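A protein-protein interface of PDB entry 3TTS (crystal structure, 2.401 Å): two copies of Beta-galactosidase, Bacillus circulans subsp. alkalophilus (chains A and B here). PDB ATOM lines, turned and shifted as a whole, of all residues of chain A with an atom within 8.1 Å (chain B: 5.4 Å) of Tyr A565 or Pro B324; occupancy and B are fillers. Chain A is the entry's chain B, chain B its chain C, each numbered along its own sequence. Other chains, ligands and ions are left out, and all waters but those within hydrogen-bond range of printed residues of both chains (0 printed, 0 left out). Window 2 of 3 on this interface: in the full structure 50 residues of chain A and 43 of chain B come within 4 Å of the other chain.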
ATOM      1  N   GLU A 515     -12.571 -15.310   3.341  1.00  0.00           N
ATOM      2  CA  GLU A 515     -11.847 -14.987   4.577  1.00  0.00           C
ATOM      3  C   GLU A 515     -10.334 -14.898   4.368  1.00  0.00           C
ATOM      4  O   GLU A 515      -9.717 -13.900   4.720  1.00  0.00           O
ATOM      5  CB  GLU A 515     -12.152 -15.996   5.688  1.00  0.00           C
ATOM      6  CG  GLU A 515     -11.314 -15.759   6.941  1.00  0.00           C
ATOM      7  CD  GLU A 515     -11.592 -16.749   8.075  1.00  0.00           C
ATOM      8  OE1 GLU A 515     -12.613 -17.469   8.034  1.00  0.00           O
ATOM      9  OE2 GLU A 515     -10.780 -16.806   9.023  1.00  0.00           O
ATOM     10  N   GLU A 516      -9.743 -15.946   3.805  1.00  0.00           N
ATOM     11  CA  GLU A 516      -8.313 -15.957   3.535  1.00  0.00           C
ATOM     12  C   GLU A 516      -8.020 -16.812   2.315  1.00  0.00           C
ATOM     13  O   GLU A 516      -8.768 -17.733   2.004  1.00  0.00           O
ATOM     14  CB  GLU A 516      -7.521 -16.464   4.746  1.00  0.00           C
ATOM     15  CG  GLU A 516      -7.801 -17.903   5.124  1.00  0.00           C
ATOM     16  CD  GLU A 516      -7.110 -18.331   6.428  1.00  0.00           C
ATOM     17  OE1 GLU A 516      -7.215 -19.524   6.784  1.00  0.00           O
ATOM     18  OE2 GLU A 516      -6.473 -17.488   7.103  1.00  0.00           O
ATOM     19  N   ILE A 517      -6.927 -16.507   1.627  1.00  0.00           N
ATOM     20  CA  ILE A 517      -6.568 -17.247   0.426  1.00  0.00           C
ATOM     21  C   ILE A 517      -5.285 -18.018   0.702  1.00  0.00           C
ATOM     22  O   ILE A 517      -4.439 -17.558   1.463  1.00  0.00           O
ATOM     23  CB  ILE A 517      -6.450 -16.298  -0.811  1.00  0.00           C
ATOM     24  CG1 ILE A 517      -6.534 -17.088  -2.125  1.00  0.00           C
ATOM     25  CG2 ILE A 517      -5.208 -15.405  -0.709  1.00  0.00           C
ATOM     26  CD1 ILE A 517      -6.611 -16.225  -3.376  1.00  0.00           C
ATOM     27  N   ASP A 518      -5.163 -19.211   0.125  1.00  0.00           N
ATOM     28  CA  ASP A 518      -3.994 -20.063   0.338  1.00  0.00           C
ATOM     29  C   ASP A 518      -3.270 -20.367  -0.981  1.00  0.00           C
ATOM     30  O   ASP A 518      -3.860 -20.939  -1.907  1.00  0.00           O
ATOM     31  CB  ASP A 518      -4.403 -21.374   1.018  1.00  0.00           C
ATOM     32  CG  ASP A 518      -3.208 -22.289   1.305  1.00  0.00           C
ATOM     33  OD1 ASP A 518      -2.128 -21.772   1.657  1.00  0.00           O
ATOM     34  OD2 ASP A 518      -3.343 -23.525   1.175  1.00  0.00           O
ATOM     35  N   ALA A 519      -1.996 -19.986  -1.065  1.00  0.00           N
ATOM     36  CA  ALA A 519      -1.199 -20.257  -2.262  1.00  0.00           C
ATOM     37  C   ALA A 519      -0.581 -21.625  -2.161  1.00  0.00           C
ATOM     38  O   ALA A 519       0.092 -21.937  -1.184  1.00  0.00           O
ATOM     39  CB  ALA A 519      -0.113 -19.220  -2.440  1.00  0.00           C
ATOM     40  N   ASN A 526      -5.655 -29.314  -4.491  1.00  0.00           N
ATOM     41  CA  ASN A 526      -6.715 -29.716  -3.591  1.00  0.00           C
ATOM     42  C   ASN A 526      -7.753 -30.353  -4.487  1.00  0.00           C
ATOM     43  O   ASN A 526      -7.490 -30.553  -5.677  1.00  0.00           O
ATOM     44  CB  ASN A 526      -7.304 -28.524  -2.847  1.00  0.00           C
ATOM     45  CG  ASN A 526      -7.948 -28.930  -1.531  1.00  0.00           C
ATOM     46  OD1 ASN A 526      -8.951 -29.655  -1.506  1.00  0.00           O
ATOM     47  ND2 ASN A 526      -7.367 -28.477  -0.431  1.00  0.00           N
ATOM     48  N   CYS A 547      -6.146 -21.383  -3.364  1.00  0.00           N
ATOM     49  CA  CYS A 547      -7.405 -21.848  -2.791  1.00  0.00           C
ATOM     50  C   CYS A 547      -7.981 -20.838  -1.817  1.00  0.00           C
ATOM     51  O   CYS A 547      -7.408 -20.568  -0.771  1.00  0.00           O
ATOM     52  CB  CYS A 547      -7.232 -23.211  -2.118  1.00  0.00           C
ATOM     53  SG  CYS A 547      -6.816 -24.526  -3.272  1.00  0.00           S
ATOM     54  N   ASP A 548      -9.130 -20.287  -2.166  1.00  0.00           N
ATOM     55  CA  ASP A 548      -9.771 -19.273  -1.347  1.00  0.00           C
ATOM     56  C   ASP A 548     -10.655 -19.953  -0.305  1.00  0.00           C
ATOM     57  O   ASP A 548     -11.360 -20.917  -0.610  1.00  0.00           O
ATOM     58  CB  ASP A 548     -10.612 -18.371  -2.243  1.00  0.00           C
ATOM     59  CG  ASP A 548     -10.551 -16.918  -1.831  1.00  0.00           C
ATOM     60  OD1 ASP A 548      -9.943 -16.633  -0.770  1.00  0.00           O
ATOM     61  OD2 ASP A 548     -11.116 -16.066  -2.563  1.00  0.00           O
ATOM     62  N   VAL A 549     -10.604 -19.458   0.926  1.00  0.00           N
ATOM     63  CA  VAL A 549     -11.361 -20.032   2.026  1.00  0.00           C
ATOM     64  C   VAL A 549     -12.546 -19.136   2.324  1.00  0.00           C
ATOM     65  O   VAL A 549     -12.399 -18.066   2.909  1.00  0.00           O
ATOM     66  CB  VAL A 549     -10.490 -20.183   3.295  1.00  0.00           C
ATOM     67  CG1 VAL A 549     -11.300 -20.797   4.452  1.00  0.00           C
ATOM     68  CG2 VAL A 549      -9.272 -21.030   2.995  1.00  0.00           C
ATOM     69  N   TYR A 561     -14.224 -28.303  -0.893  1.00  0.00           N
ATOM     70  CA  TYR A 561     -12.860 -28.822  -1.035  1.00  0.00           C
ATOM     71  C   TYR A 561     -12.786 -30.217  -0.459  1.00  0.00           C
ATOM     72  O   TYR A 561     -13.460 -30.522   0.523  1.00  0.00           O
ATOM     73  CB  TYR A 561     -11.834 -27.952  -0.298  1.00  0.00           C
ATOM     74  CG  TYR A 561     -11.560 -26.591  -0.897  1.00  0.00           C
ATOM     75  CD1 TYR A 561     -12.135 -25.443  -0.346  1.00  0.00           C
ATOM     76  CD2 TYR A 561     -10.703 -26.442  -1.984  1.00  0.00           C
ATOM     77  CE1 TYR A 561     -11.882 -24.193  -0.866  1.00  0.00           C
ATOM     78  CE2 TYR A 561     -10.444 -25.181  -2.523  1.00  0.00           C
ATOM     79  CZ  TYR A 561     -11.040 -24.061  -1.957  1.00  0.00           C
ATOM     80  OH  TYR A 561     -10.798 -22.803  -2.465  1.00  0.00           O
ATOM     81  N   GLY A 562     -11.942 -31.055  -1.039  1.00  0.00           N
ATOM     82  CA  GLY A 562     -11.807 -32.413  -0.556  1.00  0.00           C
ATOM     83  C   GLY A 562     -10.585 -32.696   0.299  1.00  0.00           C
ATOM     84  O   GLY A 562     -10.364 -33.839   0.696  1.00  0.00           O
ATOM     85  N   ALA A 563      -9.785 -31.675   0.593  1.00  0.00           N
ATOM     86  CA  ALA A 563      -8.575 -31.898   1.383  1.00  0.00           C
ATOM     87  C   ALA A 563      -8.081 -30.667   2.130  1.00  0.00           C
ATOM     88  O   ALA A 563      -8.631 -29.575   1.988  1.00  0.00           O
ATOM     89  CB  ALA A 563      -7.465 -32.468   0.505  1.00  0.00           C
ATOM     90  N   ASP A 564      -7.038 -30.874   2.934  1.00  0.00           N
ATOM     91  CA  ASP A 564      -6.368 -29.814   3.682  1.00  0.00           C
ATOM     92  C   ASP A 564      -7.231 -29.242   4.794  1.00  0.00           C
ATOM     93  O   ASP A 564      -8.364 -29.684   4.991  1.00  0.00           O
ATOM     94  CB  ASP A 564      -5.878 -28.697   2.758  1.00  0.00           C
ATOM     95  CG  ASP A 564      -4.505 -28.161   3.172  1.00  0.00           C
ATOM     96  OD1 ASP A 564      -4.226 -28.087   4.399  1.00  0.00           O
ATOM     97  OD2 ASP A 564      -3.698 -27.838   2.266  1.00  0.00           O
ATOM     98  N   TYR A 565      -6.701 -28.254   5.512  1.00  0.00           N
ATOM     99  CA  TYR A 565      -7.393 -27.741   6.694  1.00  0.00           C
ATOM    100  C   TYR A 565      -8.722 -27.085   6.363  1.00  0.00           C
ATOM    101  O   TYR A 565      -9.548 -26.892   7.254  1.00  0.00           O
ATOM    102  CB  TYR A 565      -6.516 -26.802   7.533  1.00  0.00           C
ATOM    103  CG  TYR A 565      -6.392 -25.375   7.026  1.00  0.00           C
ATOM    104  CD1 TYR A 565      -5.364 -25.017   6.157  1.00  0.00           C
ATOM    105  CD2 TYR A 565      -7.276 -24.380   7.444  1.00  0.00           C
ATOM    106  CE1 TYR A 565      -5.219 -23.719   5.701  1.00  0.00           C
ATOM    107  CE2 TYR A 565      -7.148 -23.068   6.986  1.00  0.00           C
ATOM    108  CZ  TYR A 565      -6.104 -22.741   6.116  1.00  0.00           C
ATOM    109  OH  TYR A 565      -5.937 -21.447   5.641  1.00  0.00           O
ATOM    110  N   TYR A 566      -8.924 -26.737   5.090  1.00  0.00           N
ATOM    111  CA  TYR A 566     -10.203 -26.179   4.658  1.00  0.00           C
ATOM    112  C   TYR A 566     -11.089 -27.194   3.925  1.00  0.00           C
ATOM    113  O   TYR A 566     -12.045 -26.826   3.235  1.00  0.00           O
ATOM    114  CB  TYR A 566     -10.013 -24.898   3.838  1.00  0.00           C
ATOM    115  CG  TYR A 566      -8.834 -24.907   2.900  1.00  0.00           C
ATOM    116  CD1 TYR A 566      -8.986 -25.269   1.575  1.00  0.00           C
ATOM    117  CD2 TYR A 566      -7.568 -24.527   3.336  1.00  0.00           C
ATOM    118  CE1 TYR A 566      -7.909 -25.271   0.706  1.00  0.00           C
ATOM    119  CE2 TYR A 566      -6.490 -24.523   2.471  1.00  0.00           C
ATOM    120  CZ  TYR A 566      -6.667 -24.895   1.157  1.00  0.00           C
ATOM    121  OH  TYR A 566      -5.603 -24.896   0.282  1.00  0.00           O
ATOM    122  N   LYS A 567     -10.769 -28.472   4.105  1.00  0.00           N
ATOM    123  CA  LYS A 567     -11.616 -29.568   3.638  1.00  0.00           C
ATOM    124  C   LYS A 567     -13.043 -29.420   4.148  1.00  0.00           C
ATOM    125  O   LYS A 567     -13.268 -29.203   5.346  1.00  0.00           O
ATOM    126  CB  LYS A 567     -11.056 -30.911   4.111  1.00  0.00           C
ATOM    127  CG  LYS A 567     -11.932 -32.102   3.766  1.00  0.00           C
ATOM    128  CD  LYS A 567     -11.364 -33.395   4.343  1.00  0.00           C
ATOM    129  CE  LYS A 567     -12.039 -34.624   3.732  1.00  0.00           C
ATOM    130  NZ  LYS A 567     -11.379 -35.896   4.169  1.00  0.00           N
ATOM    131  N   GLY A 568     -14.005 -29.537   3.236  1.00  0.00           N
ATOM    132  CA  GLY A 568     -15.409 -29.444   3.595  1.00  0.00           C
ATOM    133  C   GLY A 568     -15.963 -28.031   3.575  1.00  0.00           C
ATOM    134  O   GLY A 568     -17.114 -27.819   3.956  1.00  0.00           O
ATOM    135  N   THR A 569     -15.151 -27.061   3.142  1.00  0.00           N
ATOM    136  CA  THR A 569     -15.631 -25.679   2.980  1.00  0.00           C
ATOM    137  C   THR A 569     -15.944 -25.371   1.509  1.00  0.00           C
ATOM    138  O   THR A 569     -15.480 -26.075   0.620  1.00  0.00           O
ATOM    139  CB  THR A 569     -14.654 -24.631   3.593  1.00  0.00           C
ATOM    140  OG1 THR A 569     -13.383 -24.671   2.928  1.00  0.00           O
ATOM    141  CG2 THR A 569     -14.451 -24.903   5.081  1.00  0.00           C
ATOM    142  N   ALA B 321      -0.705 -20.299   3.483  1.00  0.00           N
ATOM    143  CA  ALA B 321      -1.213 -19.959   4.801  1.00  0.00           C
ATOM    144  C   ALA B 321      -0.525 -20.830   5.852  1.00  0.00           C
ATOM    145  O   ALA B 321      -0.131 -21.963   5.586  1.00  0.00           O
ATOM    146  CB  ALA B 321      -2.726 -20.123   4.849  1.00  0.00           C
ATOM    147  N   LYS B 322      -0.361 -20.280   7.044  1.00  0.00           N
ATOM    148  CA  LYS B 322       0.198 -21.024   8.150  1.00  0.00           C
ATOM    149  C   LYS B 322      -0.911 -21.931   8.698  1.00  0.00           C
ATOM    150  O   LYS B 322      -1.917 -21.434   9.189  1.00  0.00           O
ATOM    151  CB  LYS B 322       0.676 -20.035   9.213  1.00  0.00           C
ATOM    152  CG  LYS B 322       1.833 -20.534  10.027  1.00  0.00           C
ATOM    153  CD  LYS B 322       3.043 -19.628   9.895  1.00  0.00           C
ATOM    154  CE  LYS B 322       2.930 -18.384  10.765  1.00  0.00           C
ATOM    155  NZ  LYS B 322       4.276 -17.746  10.954  1.00  0.00           N
ATOM    156  N   ARG B 323      -0.746 -23.249   8.590  1.00  0.00           N
ATOM    157  CA  ARG B 323      -1.787 -24.190   9.011  1.00  0.00           C
ATOM    158  C   ARG B 323      -2.150 -23.988  10.482  1.00  0.00           C
ATOM    159  O   ARG B 323      -1.356 -23.452  11.256  1.00  0.00           O
ATOM    160  CB  ARG B 323      -1.345 -25.649   8.806  1.00  0.00           C
ATOM    161  CG  ARG B 323      -0.621 -25.955   7.502  1.00  0.00           C
ATOM    162  CD  ARG B 323      -1.538 -26.087   6.303  1.00  0.00           C
ATOM    163  NE  ARG B 323      -1.424 -24.902   5.474  1.00  0.00           N
ATOM    164  CZ  ARG B 323      -1.724 -24.836   4.182  1.00  0.00           C
ATOM    165  NH1 ARG B 323      -2.156 -25.899   3.529  1.00  0.00           N
ATOM    166  NH2 ARG B 323      -1.570 -23.687   3.540  1.00  0.00           N
ATOM    167  N   PRO B 324      -3.347 -24.443  10.883  1.00  0.00           N
ATOM    168  CA  PRO B 324      -3.807 -24.258  12.271  1.00  0.00           C
ATOM    169  C   PRO B 324      -2.806 -24.787  13.308  1.00  0.00           C
ATOM    170  O   PRO B 324      -2.323 -25.919  13.201  1.00  0.00           O
ATOM    171  CB  PRO B 324      -5.124 -25.061  12.319  1.00  0.00           C
ATOM    172  CG  PRO B 324      -5.606 -25.083  10.897  1.00  0.00           C
ATOM    173  CD  PRO B 324      -4.342 -25.153  10.056  1.00  0.00           C
ATOM    174  N   GLY B 325      -2.492 -23.959  14.297  1.00  0.00           N
ATOM    175  CA  GLY B 325      -1.527 -24.316  15.324  1.00  0.00           C
ATOM    176  C   GLY B 325      -0.082 -23.929  15.028  1.00  0.00           C
ATOM    177  O   GLY B 325       0.722 -23.735  15.951  1.00  0.00           O
ATOM    178  N   VAL B 326       0.258 -23.806  13.747  1.00  0.00           N
ATOM    179  CA  VAL B 326       1.652 -23.580  13.365  1.00  0.00           C
ATOM    180  C   VAL B 326       2.199 -22.245  13.870  1.00  0.00           C
ATOM    181  O   VAL B 326       3.366 -22.137  14.252  1.00  0.00           O
ATOM    182  CB  VAL B 326       1.846 -23.724  11.852  1.00  0.00           C
ATOM    183  CG1 VAL B 326       3.268 -23.348  11.453  1.00  0.00           C
ATOM    184  CG2 VAL B 326       1.524 -25.152  11.428  1.00  0.00           C
ATOM    185  N   ARG B 371     -10.057 -16.890  11.817  1.00  0.00           N
ATOM    186  CA  ARG B 371      -9.129 -17.931  12.205  1.00  0.00           C
ATOM    187  C   ARG B 371      -7.797 -17.338  12.706  1.00  0.00           C
ATOM    188  O   ARG B 371      -7.403 -17.573  13.857  1.00  0.00           O
ATOM    189  CB  ARG B 371      -8.898 -18.874  11.029  1.00  0.00           C
ATOM    190  CG  ARG B 371      -8.159 -20.116  11.398  1.00  0.00           C
ATOM    191  CD  ARG B 371      -7.650 -20.829  10.171  1.00  0.00           C
ATOM    192  NE  ARG B 371      -6.276 -21.209  10.434  1.00  0.00           N
ATOM    193  CZ  ARG B 371      -5.221 -20.792   9.752  1.00  0.00           C
ATOM    194  NH1 ARG B 371      -5.350 -20.006   8.695  1.00  0.00           N
ATOM    195  NH2 ARG B 371      -4.027 -21.197  10.135  1.00  0.00           N
ATOM    196  N   GLU B 375      -6.381 -17.744  16.683  1.00  0.00           N
ATOM    197  CA  GLU B 375      -5.110 -18.379  17.031  1.00  0.00           C
ATOM    198  C   GLU B 375      -4.183 -17.434  17.805  1.00  0.00           C
ATOM    199  O   GLU B 375      -3.509 -17.851  18.749  1.00  0.00           O
ATOM    200  CB  GLU B 375      -4.443 -18.955  15.773  1.00  0.00           C
ATOM    201  CG  GLU B 375      -5.340 -19.992  15.063  1.00  0.00           C
ATOM    202  CD  GLU B 375      -4.612 -20.796  13.995  1.00  0.00           C
ATOM    203  OE1 GLU B 375      -3.383 -20.979  14.128  1.00  0.00           O
ATOM    204  OE2 GLU B 375      -5.266 -21.231  13.011  1.00  0.00           O
ATOM    205  N   ARG B 667       1.067 -30.625  15.912  1.00  0.00           N
ATOM    206  CA  ARG B 667       1.414 -29.211  16.016  1.00  0.00           C
ATOM    207  C   ARG B 667       1.453 -28.741  17.465  1.00  0.00           C
ATOM    208  O   ARG B 667       1.349 -27.543  17.729  1.00  0.00           O
ATOM    209  CB  ARG B 667       0.425 -28.344  15.225  1.00  0.00           C
ATOM    210  CG  ARG B 667       0.886 -27.995  13.822  1.00  0.00           C
ATOM    211  CD  ARG B 667       0.195 -28.827  12.748  1.00  0.00           C
ATOM    212  NE  ARG B 667       1.035 -28.933  11.560  1.00  0.00           N
ATOM    213  CZ  ARG B 667       0.588 -29.150  10.325  1.00  0.00           C
ATOM    214  NH1 ARG B 667      -0.713 -29.278  10.079  1.00  0.00           N
ATOM    215  NH2 ARG B 667       1.456 -29.235   9.324  1.00  0.00           N
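The side-chain carboxylate (OE2) of Glu A515 lies within hydrogen-bond range of the backbone NH (N) of Arg B371 (2.9 Å). OE1 of Glu A516 is in salt-bridge range of NH1 of Arg B371. The side-chain carboxylate (OD1) of Asp A518 sits at hydrogen-bond distance from the backbone NH (N) of Ala B321 (2.7 Å). The guanidinium group (NH2) of Arg B323 is in salt-bridge range of the side-chain carboxylate (OD1) of Asp A518, at 2.7 Å. The side-chain carboxylate (OD2) of Asp A564 lies within salt-bridge range of the guanidinium group (NH1) of Arg B323 (2.8 Å). OH of Tyr A565 is in hydrogen-bond range of NH1 of Arg B371, 3.4 Å away.
N of Glu A515 is in hydrogen-bond range of O of Val A549 (2.8 Å). The backbone carbonyl oxygen of Glu A516 is in hydrogen-bond range of the backbone NH of Val A549 (2.7 Å). The backbone carbonyl oxygen (O) of Asp A518 lies within hydrogen-bond range of the backbone NH (N) of Cys A547 (2.7 Å). The side-chain hydroxyl of Tyr A566 sits at hydrogen-bond distance from the side-chain carboxylate of Asp A518 (2.8 Å). The guanidinium group (NH2) of Arg B323 sits at hydrogen-bond distance from the backbone carbonyl oxygen (O) of Ala B321 (3.0 Å). NE of Arg B371 lies within salt-bridge range of OE2 of Glu B375 (2.8 Å).
Ala B321 touches Tyr A565 (CB to OH, 3.6 Å). Arg B323 touches Tyr A565 (CZ to CE1, 3.97 Å). Tyr A565 touches Pro B324 (CG to CD, 3.7 Å).
Of the printed residues of chain B, Glu A515 touches Arg B371 (2.9 Å). Asn A526 touches none of the printed residues of chain B. Of the printed residues of chain B, Asp A564 touches Arg B323. Of chain B, only Ala B321, Arg B323, Pro B324 and Arg B371 come within 4 Å of Tyr A565. Of chain A, only Tyr A565 comes within 4 Å of Pro B324. Gly B325 touches none of the printed residues of chain A. Printed residues of chain A within 4 Å of Arg B371: Glu A515 (2.9 Å), Glu A516 (2.7 Å) and Tyr A565 (3.4 Å).
Of the 18 printed residues of chain A, 5 touch a printed residue of chain B. Hydrophobic or aromatic side chains of chain A within 4 Å of the printed part of chain B: Tyr A565. Hydrophobic or aromatic side chains of chain B that line the printed part of chain A: Ala B321 and Pro B324. Among the printed residues, 9 pairs touch across the chains.
No position is printed for both chains. Of the 9 pairs that touch across the chains among the printed residues, none has its exchanged pair printed and touching as well.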
